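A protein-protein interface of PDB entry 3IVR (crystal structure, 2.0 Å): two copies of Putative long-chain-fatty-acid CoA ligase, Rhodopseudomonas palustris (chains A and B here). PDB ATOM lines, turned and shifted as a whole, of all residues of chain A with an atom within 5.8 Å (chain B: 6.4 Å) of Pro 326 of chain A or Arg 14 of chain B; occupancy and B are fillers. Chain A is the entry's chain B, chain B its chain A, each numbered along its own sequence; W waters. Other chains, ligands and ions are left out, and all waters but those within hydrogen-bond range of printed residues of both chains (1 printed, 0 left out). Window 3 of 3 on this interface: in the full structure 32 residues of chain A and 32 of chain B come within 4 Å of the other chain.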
ATOM      1  N   SER A 311     -15.136  27.186 -36.386  1.00  0.00           N
ATOM      2  CA  SER A 311     -14.161  26.299 -35.751  1.00  0.00           C
ATOM      3  C   SER A 311     -12.852  26.995 -35.385  1.00  0.00           C
ATOM      4  O   SER A 311     -12.295  26.762 -34.300  1.00  0.00           O
ATOM      5  CB  SER A 311     -13.853  25.112 -36.658  1.00  0.00           C
ATOM      6  OG  SER A 311     -14.957  24.254 -36.674  1.00  0.00           O
ATOM      7  N   THR A 312     -12.353  27.800 -36.329  1.00  0.00           N
ATOM      8  CA  THR A 312     -11.148  28.614 -36.171  1.00  0.00           C
ATOM      9  C   THR A 312     -11.541  30.085 -36.258  1.00  0.00           C
ATOM     10  O   THR A 312     -12.484  30.436 -36.969  1.00  0.00           O
ATOM     11  CB  THR A 312     -10.021  28.256 -37.216  1.00  0.00           C
ATOM     12  OG1 THR A 312     -10.485  28.479 -38.551  1.00  0.00           O
ATOM     13  CG2 THR A 312      -9.619  26.803 -37.096  1.00  0.00           C
ATOM     14  N   PHE A 313     -10.831  30.930 -35.512  1.00  0.00           N
ATOM     15  CA  PHE A 313     -11.191  32.331 -35.318  1.00  0.00           C
ATOM     16  C   PHE A 313      -9.976  33.111 -34.788  1.00  0.00           C
ATOM     17  O   PHE A 313      -9.272  32.624 -33.895  1.00  0.00           O
ATOM     18  CB  PHE A 313     -12.296  32.393 -34.271  1.00  0.00           C
ATOM     19  CG  PHE A 313     -13.271  33.519 -34.435  1.00  0.00           C
ATOM     20  CD1 PHE A 313     -13.654  34.272 -33.327  1.00  0.00           C
ATOM     21  CD2 PHE A 313     -13.874  33.776 -35.661  1.00  0.00           C
ATOM     22  CE1 PHE A 313     -14.602  35.298 -33.451  1.00  0.00           C
ATOM     23  CE2 PHE A 313     -14.830  34.785 -35.797  1.00  0.00           C
ATOM     24  CZ  PHE A 313     -15.192  35.555 -34.704  1.00  0.00           C
ATOM     25  N   GLY A 324      -7.611  31.917 -38.967  1.00  0.00           N
ATOM     26  CA  GLY A 324      -7.518  32.058 -37.508  1.00  0.00           C
ATOM     27  C   GLY A 324      -6.975  30.843 -36.781  1.00  0.00           C
ATOM     28  O   GLY A 324      -6.457  29.914 -37.397  1.00  0.00           O
ATOM     29  N   ARG A 325      -7.096  30.884 -35.454  1.00  0.00           N
ATOM     30  CA  ARG A 325      -6.643  29.810 -34.587  1.00  0.00           C
ATOM     31  C   ARG A 325      -7.843  28.970 -34.108  1.00  0.00           C
ATOM     32  O   ARG A 325      -8.942  29.514 -33.923  1.00  0.00           O
ATOM     33  CB  ARG A 325      -5.893  30.427 -33.396  1.00  0.00           C
ATOM     34  CG  ARG A 325      -4.595  29.723 -33.030  1.00  0.00           C
ATOM     35  CD  ARG A 325      -3.389  30.653 -33.101  1.00  0.00           C
ATOM     36  NE  ARG A 325      -3.335  31.587 -31.977  1.00  0.00           N
ATOM     37  CZ  ARG A 325      -2.262  31.816 -31.222  1.00  0.00           C
ATOM     38  NH1 ARG A 325      -1.107  31.195 -31.459  1.00  0.00           N
ATOM     39  NH2 ARG A 325      -2.350  32.691 -30.226  1.00  0.00           N
ATOM     40  N   PRO A 326      -7.642  27.631 -33.906  1.00  0.00           N
ATOM     41  CA  PRO A 326      -8.733  26.809 -33.343  1.00  0.00           C
ATOM     42  C   PRO A 326      -9.303  27.390 -32.049  1.00  0.00           C
ATOM     43  O   PRO A 326      -8.533  27.790 -31.186  1.00  0.00           O
ATOM     44  CB  PRO A 326      -8.033  25.484 -33.016  1.00  0.00           C
ATOM     45  CG  PRO A 326      -6.903  25.412 -33.998  1.00  0.00           C
ATOM     46  CD  PRO A 326      -6.439  26.810 -34.174  1.00  0.00           C
ATOM     47  N   LEU A 327     -10.630  27.452 -31.923  1.00  0.00           N
ATOM     48  CA  LEU A 327     -11.276  27.935 -30.688  1.00  0.00           C
ATOM     49  C   LEU A 327     -11.234  26.890 -29.596  1.00  0.00           C
ATOM     50  O   LEU A 327     -11.050  25.700 -29.874  1.00  0.00           O
ATOM     51  CB  LEU A 327     -12.750  28.298 -30.940  1.00  0.00           C
ATOM     52  CG  LEU A 327     -12.957  29.503 -31.837  1.00  0.00           C
ATOM     53  CD1 LEU A 327     -14.315  29.448 -32.509  1.00  0.00           C
ATOM     54  CD2 LEU A 327     -12.802  30.765 -30.983  1.00  0.00           C
ATOM     55  N   PHE A 328     -11.440  27.324 -28.352  1.00  0.00           N
ATOM     56  CA  PHE A 328     -11.684  26.376 -27.266  1.00  0.00           C
ATOM     57  C   PHE A 328     -12.896  25.481 -27.615  1.00  0.00           C
ATOM     58  O   PHE A 328     -13.839  25.930 -28.289  1.00  0.00           O
ATOM     59  CB  PHE A 328     -11.880  27.124 -25.932  1.00  0.00           C
ATOM     60  CG  PHE A 328     -11.775  26.243 -24.727  1.00  0.00           C
ATOM     61  CD1 PHE A 328     -10.525  25.892 -24.207  1.00  0.00           C
ATOM     62  CD2 PHE A 328     -12.921  25.744 -24.117  1.00  0.00           C
ATOM     63  CE1 PHE A 328     -10.426  25.059 -23.077  1.00  0.00           C
ATOM     64  CE2 PHE A 328     -12.832  24.898 -22.979  1.00  0.00           C
ATOM     65  CZ  PHE A 328     -11.573  24.569 -22.462  1.00  0.00           C
ATOM     66  N   TRP A 329     -12.819  24.216 -27.181  1.00  0.00           N
ATOM     67  CA  TRP A 329     -13.766  23.123 -27.443  1.00  0.00           C
ATOM     68  C   TRP A 329     -13.500  22.369 -28.755  1.00  0.00           C
ATOM     69  O   TRP A 329     -14.113  21.317 -28.991  1.00  0.00           O
ATOM     70  CB  TRP A 329     -15.258  23.531 -27.361  1.00  0.00           C
ATOM     71  CG  TRP A 329     -15.701  24.214 -26.071  1.00  0.00           C
ATOM     72  CD1 TRP A 329     -16.093  25.496 -25.939  1.00  0.00           C
ATOM     73  CD2 TRP A 329     -15.790  23.634 -24.769  1.00  0.00           C
ATOM     74  NE1 TRP A 329     -16.437  25.776 -24.633  1.00  0.00           N
ATOM     75  CE2 TRP A 329     -16.259  24.644 -23.891  1.00  0.00           C
ATOM     76  CE3 TRP A 329     -15.498  22.362 -24.245  1.00  0.00           C
ATOM     77  CZ2 TRP A 329     -16.455  24.427 -22.534  1.00  0.00           C
ATOM     78  CZ3 TRP A 329     -15.709  22.141 -22.899  1.00  0.00           C
ATOM     79  CH2 TRP A 329     -16.198  23.166 -22.060  1.00  0.00           C
ATOM     80  N   ARG A 330     -12.599  22.901 -29.592  1.00  0.00           N
ATOM     81  CA  ARG A 330     -12.259  22.311 -30.904  1.00  0.00           C
ATOM     82  C   ARG A 330     -10.866  21.721 -30.850  1.00  0.00           C
ATOM     83  O   ARG A 330      -9.932  22.370 -30.401  1.00  0.00           O
ATOM     84  CB  ARG A 330     -12.259  23.372 -32.022  1.00  0.00           C
ATOM     85  CG  ARG A 330     -13.640  23.844 -32.500  1.00  0.00           C
ATOM     86  CD  ARG A 330     -14.403  24.627 -31.459  1.00  0.00           C
ATOM     87  NE  ARG A 330     -15.385  25.503 -32.074  1.00  0.00           N
ATOM     88  CZ  ARG A 330     -16.108  26.401 -31.430  1.00  0.00           C
ATOM     89  NH1 ARG A 330     -15.964  26.555 -30.126  1.00  0.00           N
ATOM     90  NH2 ARG A 330     -16.980  27.139 -32.104  1.00  0.00           N
ATOM     91  N   VAL A 332      -8.436  20.591 -33.585  1.00  0.00           N
ATOM     92  CA  VAL A 332      -8.304  20.711 -35.031  1.00  0.00           C
ATOM     93  C   VAL A 332      -6.936  20.183 -35.450  1.00  0.00           C
ATOM     94  O   VAL A 332      -5.921  20.447 -34.800  1.00  0.00           O
ATOM     95  CB  VAL A 332      -8.483  22.177 -35.475  1.00  0.00           C
ATOM     96  CG1 VAL A 332      -8.485  22.321 -36.986  1.00  0.00           C
ATOM     97  CG2 VAL A 332      -9.773  22.757 -34.891  1.00  0.00           C
ATOM     98  N   PHE A 385      -1.424  24.289 -41.200  1.00  0.00           N
ATOM     99  CA  PHE A 385      -1.134  25.108 -40.026  1.00  0.00           C
ATOM    100  C   PHE A 385       0.259  25.723 -40.147  1.00  0.00           C
ATOM    101  O   PHE A 385       1.188  25.088 -40.657  1.00  0.00           O
ATOM    102  CB  PHE A 385      -1.199  24.270 -38.750  1.00  0.00           C
ATOM    103  CG  PHE A 385      -2.594  24.064 -38.220  1.00  0.00           C
ATOM    104  CD1 PHE A 385      -3.297  22.901 -38.511  1.00  0.00           C
ATOM    105  CD2 PHE A 385      -3.200  25.032 -37.417  1.00  0.00           C
ATOM    106  CE1 PHE A 385      -4.590  22.706 -38.016  1.00  0.00           C
ATOM    107  CE2 PHE A 385      -4.484  24.849 -36.921  1.00  0.00           C
ATOM    108  CZ  PHE A 385      -5.178  23.685 -37.221  1.00  0.00           C
ATOM    109  N   GLY A 389       0.105  27.964 -35.092  1.00  0.00           N
ATOM    110  CA  GLY A 389      -1.158  27.237 -35.040  1.00  0.00           C
ATOM    111  C   GLY A 389      -2.311  27.957 -35.718  1.00  0.00           C
ATOM    112  O   GLY A 389      -3.471  27.703 -35.409  1.00  0.00           O
ATOM    113  N   TYR A 390      -1.988  28.859 -36.641  1.00  0.00           N
ATOM    114  CA  TYR A 390      -2.992  29.498 -37.478  1.00  0.00           C
ATOM    115  C   TYR A 390      -3.278  28.613 -38.668  1.00  0.00           C
ATOM    116  O   TYR A 390      -2.354  28.069 -39.272  1.00  0.00           O
ATOM    117  CB  TYR A 390      -2.534  30.879 -37.945  1.00  0.00           C
ATOM    118  CG  TYR A 390      -2.566  31.917 -36.862  1.00  0.00           C
ATOM    119  CD1 TYR A 390      -3.713  32.685 -36.637  1.00  0.00           C
ATOM    120  CD2 TYR A 390      -1.462  32.123 -36.049  1.00  0.00           C
ATOM    121  CE1 TYR A 390      -3.747  33.633 -35.639  1.00  0.00           C
ATOM    122  CE2 TYR A 390      -1.481  33.064 -35.042  1.00  0.00           C
ATOM    123  CZ  TYR A 390      -2.620  33.816 -34.841  1.00  0.00           C
ATOM    124  OH  TYR A 390      -2.625  34.740 -33.838  1.00  0.00           O
ATOM    125  N   LEU A 391      -4.558  28.463 -38.995  1.00  0.00           N
ATOM    126  CA  LEU A 391      -4.958  27.640 -40.121  1.00  0.00           C
ATOM    127  C   LEU A 391      -5.064  28.475 -41.392  1.00  0.00           C
ATOM    128  O   LEU A 391      -5.600  29.586 -41.383  1.00  0.00           O
ATOM    129  CB  LEU A 391      -6.285  26.931 -39.832  1.00  0.00           C
ATOM    130  CG  LEU A 391      -6.956  26.069 -40.916  1.00  0.00           C
ATOM    131  CD1 LEU A 391      -6.096  24.863 -41.325  1.00  0.00           C
ATOM    132  CD2 LEU A 391      -8.328  25.618 -40.434  1.00  0.00           C
ATOM    133  N   PHE B   6     -14.102  16.714 -25.566  1.00  0.00           N
ATOM    134  CA  PHE B   6     -13.010  17.626 -25.322  1.00  0.00           C
ATOM    135  C   PHE B   6     -12.790  17.562 -23.805  1.00  0.00           C
ATOM    136  O   PHE B   6     -13.689  17.868 -23.022  1.00  0.00           O
ATOM    137  CB  PHE B   6     -13.409  19.030 -25.776  1.00  0.00           C
ATOM    138  CG  PHE B   6     -12.296  20.048 -25.741  1.00  0.00           C
ATOM    139  CD1 PHE B   6     -11.531  20.289 -26.877  1.00  0.00           C
ATOM    140  CD2 PHE B   6     -12.054  20.810 -24.595  1.00  0.00           C
ATOM    141  CE1 PHE B   6     -10.532  21.244 -26.881  1.00  0.00           C
ATOM    142  CE2 PHE B   6     -11.028  21.744 -24.586  1.00  0.00           C
ATOM    143  CZ  PHE B   6     -10.273  21.978 -25.739  1.00  0.00           C
ATOM    144  N   ALA B   9      -7.220  16.762 -21.158  1.00  0.00           N
ATOM    145  CA  ALA B   9      -6.140  16.292 -22.033  1.00  0.00           C
ATOM    146  C   ALA B   9      -6.033  17.172 -23.259  1.00  0.00           C
ATOM    147  O   ALA B   9      -4.933  17.521 -23.684  1.00  0.00           O
ATOM    148  CB  ALA B   9      -6.371  14.851 -22.459  1.00  0.00           C
ATOM    149  N   ASP B  10      -7.185  17.528 -23.823  1.00  0.00           N
ATOM    150  CA  ASP B  10      -7.235  18.355 -25.019  1.00  0.00           C
ATOM    151  C   ASP B  10      -6.802  19.790 -24.753  1.00  0.00           C
ATOM    152  O   ASP B  10      -6.251  20.432 -25.633  1.00  0.00           O
ATOM    153  CB  ASP B  10      -8.630  18.296 -25.660  1.00  0.00           C
ATOM    154  CG  ASP B  10      -8.990  16.896 -26.101  1.00  0.00           C
ATOM    155  OD1 ASP B  10      -8.294  16.342 -26.985  1.00  0.00           O
ATOM    156  OD2 ASP B  10      -9.949  16.333 -25.550  1.00  0.00           O
ATOM    157  N   VAL B  11      -7.032  20.278 -23.535  1.00  0.00           N
ATOM    158  CA  VAL B  11      -6.523  21.590 -23.104  1.00  0.00           C
ATOM    159  C   VAL B  11      -4.988  21.623 -23.025  1.00  0.00           C
ATOM    160  O   VAL B  11      -4.358  22.583 -23.487  1.00  0.00           O
ATOM    161  CB  VAL B  11      -7.085  21.959 -21.712  1.00  0.00           C
ATOM    162  CG1 VAL B  11      -6.468  23.229 -21.193  1.00  0.00           C
ATOM    163  CG2 VAL B  11      -8.598  22.035 -21.772  1.00  0.00           C
ATOM    164  N   TYR B  12      -4.399  20.567 -22.451  1.00  0.00           N
ATOM    165  CA  TYR B  12      -2.952  20.486 -22.295  1.00  0.00           C
ATOM    166  C   TYR B  12      -2.290  20.447 -23.666  1.00  0.00           C
ATOM    167  O   TYR B  12      -1.273  21.120 -23.892  1.00  0.00           O
ATOM    168  CB  TYR B  12      -2.536  19.264 -21.470  1.00  0.00           C
ATOM    169  CG  TYR B  12      -3.189  19.118 -20.098  1.00  0.00           C
ATOM    170  CD1 TYR B  12      -3.516  20.228 -19.322  1.00  0.00           C
ATOM    171  CD2 TYR B  12      -3.447  17.851 -19.578  1.00  0.00           C
ATOM    172  CE1 TYR B  12      -4.114  20.077 -18.068  1.00  0.00           C
ATOM    173  CE2 TYR B  12      -4.053  17.688 -18.330  1.00  0.00           C
ATOM    174  CZ  TYR B  12      -4.361  18.805 -17.577  1.00  0.00           C
ATOM    175  OH  TYR B  12      -4.952  18.656 -16.339  1.00  0.00           O
ATOM    176  N   ARG B  13      -2.901  19.700 -24.586  1.00  0.00           N
ATOM    177  CA  ARG B  13      -2.381  19.582 -25.951  1.00  0.00           C
ATOM    178  C   ARG B  13      -2.602  20.874 -26.722  1.00  0.00           C
ATOM    179  O   ARG B  13      -1.763  21.276 -27.516  1.00  0.00           O
ATOM    180  CB  ARG B  13      -3.008  18.387 -26.681  1.00  0.00           C
ATOM    181  CG  ARG B  13      -2.608  17.043 -26.095  1.00  0.00           C
ATOM    182  CD  ARG B  13      -3.211  15.861 -26.848  1.00  0.00           C
ATOM    183  NE  ARG B  13      -3.194  14.666 -26.009  1.00  0.00           N
ATOM    184  CZ  ARG B  13      -4.273  14.056 -25.526  1.00  0.00           C
ATOM    185  NH1 ARG B  13      -5.489  14.505 -25.826  1.00  0.00           N
ATOM    186  NH2 ARG B  13      -4.130  12.977 -24.756  1.00  0.00           N
ATOM    187  N   ARG B  14      -3.736  21.515 -26.472  1.00  0.00           N
ATOM    188  CA  ARG B  14      -4.038  22.815 -27.048  1.00  0.00           C
ATOM    189  C   ARG B  14      -2.994  23.847 -26.626  1.00  0.00           C
ATOM    190  O   ARG B  14      -2.448  24.550 -27.472  1.00  0.00           O
ATOM    191  CB  ARG B  14      -5.433  23.272 -26.609  1.00  0.00           C
ATOM    192  CG  ARG B  14      -5.767  24.685 -26.976  1.00  0.00           C
ATOM    193  CD  ARG B  14      -7.197  25.035 -26.615  1.00  0.00           C
ATOM    194  NE  ARG B  14      -7.374  26.489 -26.561  1.00  0.00           N
ATOM    195  CZ  ARG B  14      -7.708  27.239 -27.601  1.00  0.00           C
ATOM    196  NH1 ARG B  14      -7.848  28.541 -27.461  1.00  0.00           N
ATOM    197  NH2 ARG B  14      -7.904  26.685 -28.786  1.00  0.00           N
ATOM    198  N   ASN B  15      -2.727  23.927 -25.318  1.00  0.00           N
ATOM    199  CA  ASN B  15      -1.759  24.869 -24.764  1.00  0.00           C
ATOM    200  C   ASN B  15      -0.335  24.609 -25.238  1.00  0.00           C
ATOM    201  O   ASN B  15       0.378  25.551 -25.574  1.00  0.00           O
ATOM    202  CB  ASN B  15      -1.840  24.898 -23.235  1.00  0.00           C
ATOM    203  CG  ASN B  15      -3.092  25.587 -22.740  1.00  0.00           C
ATOM    204  OD1 ASN B  15      -3.729  26.347 -23.471  1.00  0.00           O
ATOM    205  ND2 ASN B  15      -3.451  25.322 -21.499  1.00  0.00           N
ATOM    206  N   ALA B  16       0.052  23.334 -25.313  1.00  0.00           N
ATOM    207  CA  ALA B  16       1.330  22.937 -25.925  1.00  0.00           C
ATOM    208  C   ALA B  16       1.424  23.288 -27.413  1.00  0.00           C
ATOM    209  O   ALA B  16       2.514  23.516 -27.920  1.00  0.00           O
ATOM    210  CB  ALA B  16       1.599  21.457 -25.711  1.00  0.00           C
ATOM    211  N   ALA B  17       0.285  23.352 -28.104  1.00  0.00           N
ATOM    212  CA  ALA B  17       0.287  23.686 -29.523  1.00  0.00           C
ATOM    213  C   ALA B  17       0.248  25.193 -29.764  1.00  0.00           C
ATOM    214  O   ALA B  17       0.982  25.697 -30.608  1.00  0.00           O
ATOM    215  CB  ALA B  17      -0.850  22.995 -30.249  1.00  0.00           C
ATOM    216  N   LEU B  18      -0.594  25.906 -29.017  1.00  0.00           N
ATOM    217  CA  LEU B  18      -0.811  27.334 -29.263  1.00  0.00           C
ATOM    218  C   LEU B  18       0.115  28.235 -28.476  1.00  0.00           C
ATOM    219  O   LEU B  18       0.505  29.287 -28.980  1.00  0.00           O
ATOM    220  CB  LEU B  18      -2.269  27.737 -29.022  1.00  0.00           C
ATOM    221  CG  LEU B  18      -3.370  27.002 -29.789  1.00  0.00           C
ATOM    222  CD1 LEU B  18      -4.682  27.734 -29.631  1.00  0.00           C
ATOM    223  CD2 LEU B  18      -3.011  26.851 -31.262  1.00  0.00           C
ATOM    224  N   PHE B  19       0.465  27.830 -27.246  1.00  0.00           N
ATOM    225  CA  PHE B  19       1.296  28.652 -26.358  1.00  0.00           C
ATOM    226  C   PHE B  19       2.476  27.878 -25.729  1.00  0.00           C
ATOM    227  O   PHE B  19       2.663  27.964 -24.510  1.00  0.00           O
ATOM    228  CB  PHE B  19       0.444  29.258 -25.215  1.00  0.00           C
ATOM    229  CG  PHE B  19      -0.960  29.647 -25.617  1.00  0.00           C
ATOM    230  CD1 PHE B  19      -1.189  30.753 -26.428  1.00  0.00           C
ATOM    231  CD2 PHE B  19      -2.056  28.903 -25.167  1.00  0.00           C
ATOM    232  CE1 PHE B  19      -2.491  31.103 -26.810  1.00  0.00           C
ATOM    233  CE2 PHE B  19      -3.373  29.245 -25.533  1.00  0.00           C
ATOM    234  CZ  PHE B  19      -3.587  30.349 -26.358  1.00  0.00           C
ATOM    235  N   PRO B  20       3.279  27.135 -26.538  1.00  0.00           N
ATOM    236  CA  PRO B  20       4.226  26.179 -25.944  1.00  0.00           C
ATOM    237  C   PRO B  20       5.257  26.789 -24.984  1.00  0.00           C
ATOM    238  O   PRO B  20       5.577  26.186 -23.953  1.00  0.00           O
ATOM    239  CB  PRO B  20       4.943  25.585 -27.168  1.00  0.00           C
ATOM    240  CG  PRO B  20       4.762  26.602 -28.265  1.00  0.00           C
ATOM    241  CD  PRO B  20       3.390  27.150 -28.013  1.00  0.00           C
ATOM    242  N   LEU B  38       3.011  19.463 -20.545  1.00  0.00           N
ATOM    243  CA  LEU B  38       2.439  18.322 -21.253  1.00  0.00           C
ATOM    244  C   LEU B  38       3.403  17.128 -21.228  1.00  0.00           C
ATOM    245  O   LEU B  38       2.983  16.000 -20.970  1.00  0.00           O
ATOM    246  CB  LEU B  38       2.049  18.676 -22.707  1.00  0.00           C
ATOM    247  CG  LEU B  38       1.434  17.517 -23.509  1.00  0.00           C
ATOM    248  CD1 LEU B  38       0.123  16.995 -22.896  1.00  0.00           C
ATOM    249  CD2 LEU B  38       1.239  17.851 -24.970  1.00  0.00           C
ATOM    250  N   GLN B 224      -7.104  26.486 -18.745  1.00  0.00           N
ATOM    251  CA  GLN B 224      -7.946  26.489 -19.949  1.00  0.00           C
ATOM    252  C   GLN B 224      -7.885  27.782 -20.824  1.00  0.00           C
ATOM    253  O   GLN B 224      -8.080  27.720 -22.034  1.00  0.00           O
ATOM    254  CB  GLN B 224      -9.344  25.937 -19.678  1.00  0.00           C
ATOM    255  CG  GLN B 224     -10.298  26.757 -18.901  1.00  0.00           C
ATOM    256  CD  GLN B 224     -11.569  25.968 -18.627  1.00  0.00           C
ATOM    257  OE1 GLN B 224     -11.589  25.072 -17.787  1.00  0.00           O
ATOM    258  NE2 GLN B 224     -12.631  26.286 -19.359  1.00  0.00           N
ATOM    259  N   ALA B 225      -7.525  28.919 -20.221  1.00  0.00           N
ATOM    260  CA  ALA B 225      -7.254  30.157 -20.966  1.00  0.00           C
ATOM    261  C   ALA B 225      -5.843  30.180 -21.587  1.00  0.00           C
ATOM    262  O   ALA B 225      -5.532  31.041 -22.414  1.00  0.00           O
ATOM    263  CB  ALA B 225      -7.455  31.379 -20.068  1.00  0.00           C
HETATM  264  O   HOH W   1      -7.991  24.050 -29.526  1.00  0.00           O
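Printed residues of chain A that touch a printed residue of chain B: Arg 325, Pro 326, Leu 327, Phe 328, Trp 329 and Arg 330. Printed residues of chain B that touch a printed residue of chain A: Phe 6, Val 11, Arg 14, Leu 18, Phe 19 and Gln 224. Among the printed residues, no Asp or Glu carboxylate lies within 4 Å of a Lys or Arg side-chain nitrogen of the other chain.
Arg 325 of chain A touches Leu 18 of chain B. Arg 325 of chain A touches Phe 19 of chain B (NH2 to CE1, 3.8 Å). Phe 328 of chain A touches Phe 6 of chain B (CZ to CE2, 3.6 Å). Phe 328 of chain A touches Val 11 of chain B (CE1 to CG2, 3.8 Å). Phe 328 of chain A touches Arg 14 of chain B (N to NH2, 3.6 Å). CE1 of Phe 328 of chain A touches CB of Gln 224 of chain B, 3.7 Å away. Trp 329 of chain A touches Phe 6 of chain B. Phe 6 of chain B touches Arg 330 of chain A (CE1 to O, 3.7 Å).
Water W1 lies within hydrogen-bond range of O of Arg 330 of chain A (2.7 Å), NH2 of Arg 14 of chain B (2.7 Å) and O of Leu 327 of chain A (3.5 Å).
Gly 324 of chain A touches none of the printed residues of chain B. Of the printed residues of chain B, Arg 325 of chain A touches Leu 18 (3.5 Å) and Phe 19 (3.8 Å). Printed residues of chain B within 4 Å of Pro 326 of chain A: Arg 14 (2.7 Å). Of the printed residues of chain B, Phe 328 of chain A touches Phe 6 (3.6 Å), Val 11 (3.8 Å), Arg 14 (3.6 Å) and Gln 224 (3.7 Å). Printed residues of chain B within 4 Å of Arg 330 of chain A: Phe 6 (3.7 Å). Tyr 390 of chain A touches none of the printed residues of chain B. Printed residues of chain A within 4 Å of Val 11 of chain B: Phe 328 (3.8 Å). Printed residues of chain A within 4 Å of Arg 14 of chain B: Pro 326, Leu 327 and Phe 328. The nearest residue of chain B that does not touch Pro 326 of chain A is Leu 18 of chain B (4.2 Å). The nearest printed residue of chain A that does not touch Arg 14 of chain B is Arg 330 of chain A (5.0 Å).
NH2 of Arg 14 of chain B is in hydrogen-bond range of O of Pro 326 of chain A (2.7 Å). The guanidinium group (NH2) of Arg 14 of chain B sits close to the backbone carbonyl oxygen (O) of Leu 327 of chain A, 3.5 Å away.
No position is printed for both chains. Of the 10 pairs that touch across the chains among the printed residues, none has its exchanged pair printed and touching as well.
The backbone carbonyl oxygen of Ser 311 of chain A is in hydrogen-bond range of the backbone NH of Leu 327 of chain A (3.0 Å). N of Phe 313 of chain A sits at hydrogen-bond distance from O of Arg 325 of chain A, 2.8 Å away. The backbone carbonyl oxygen of Phe 328 of chain A is in hydrogen-bond range of the guanidinium group of Arg 330 of chain A (2.9 Å).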
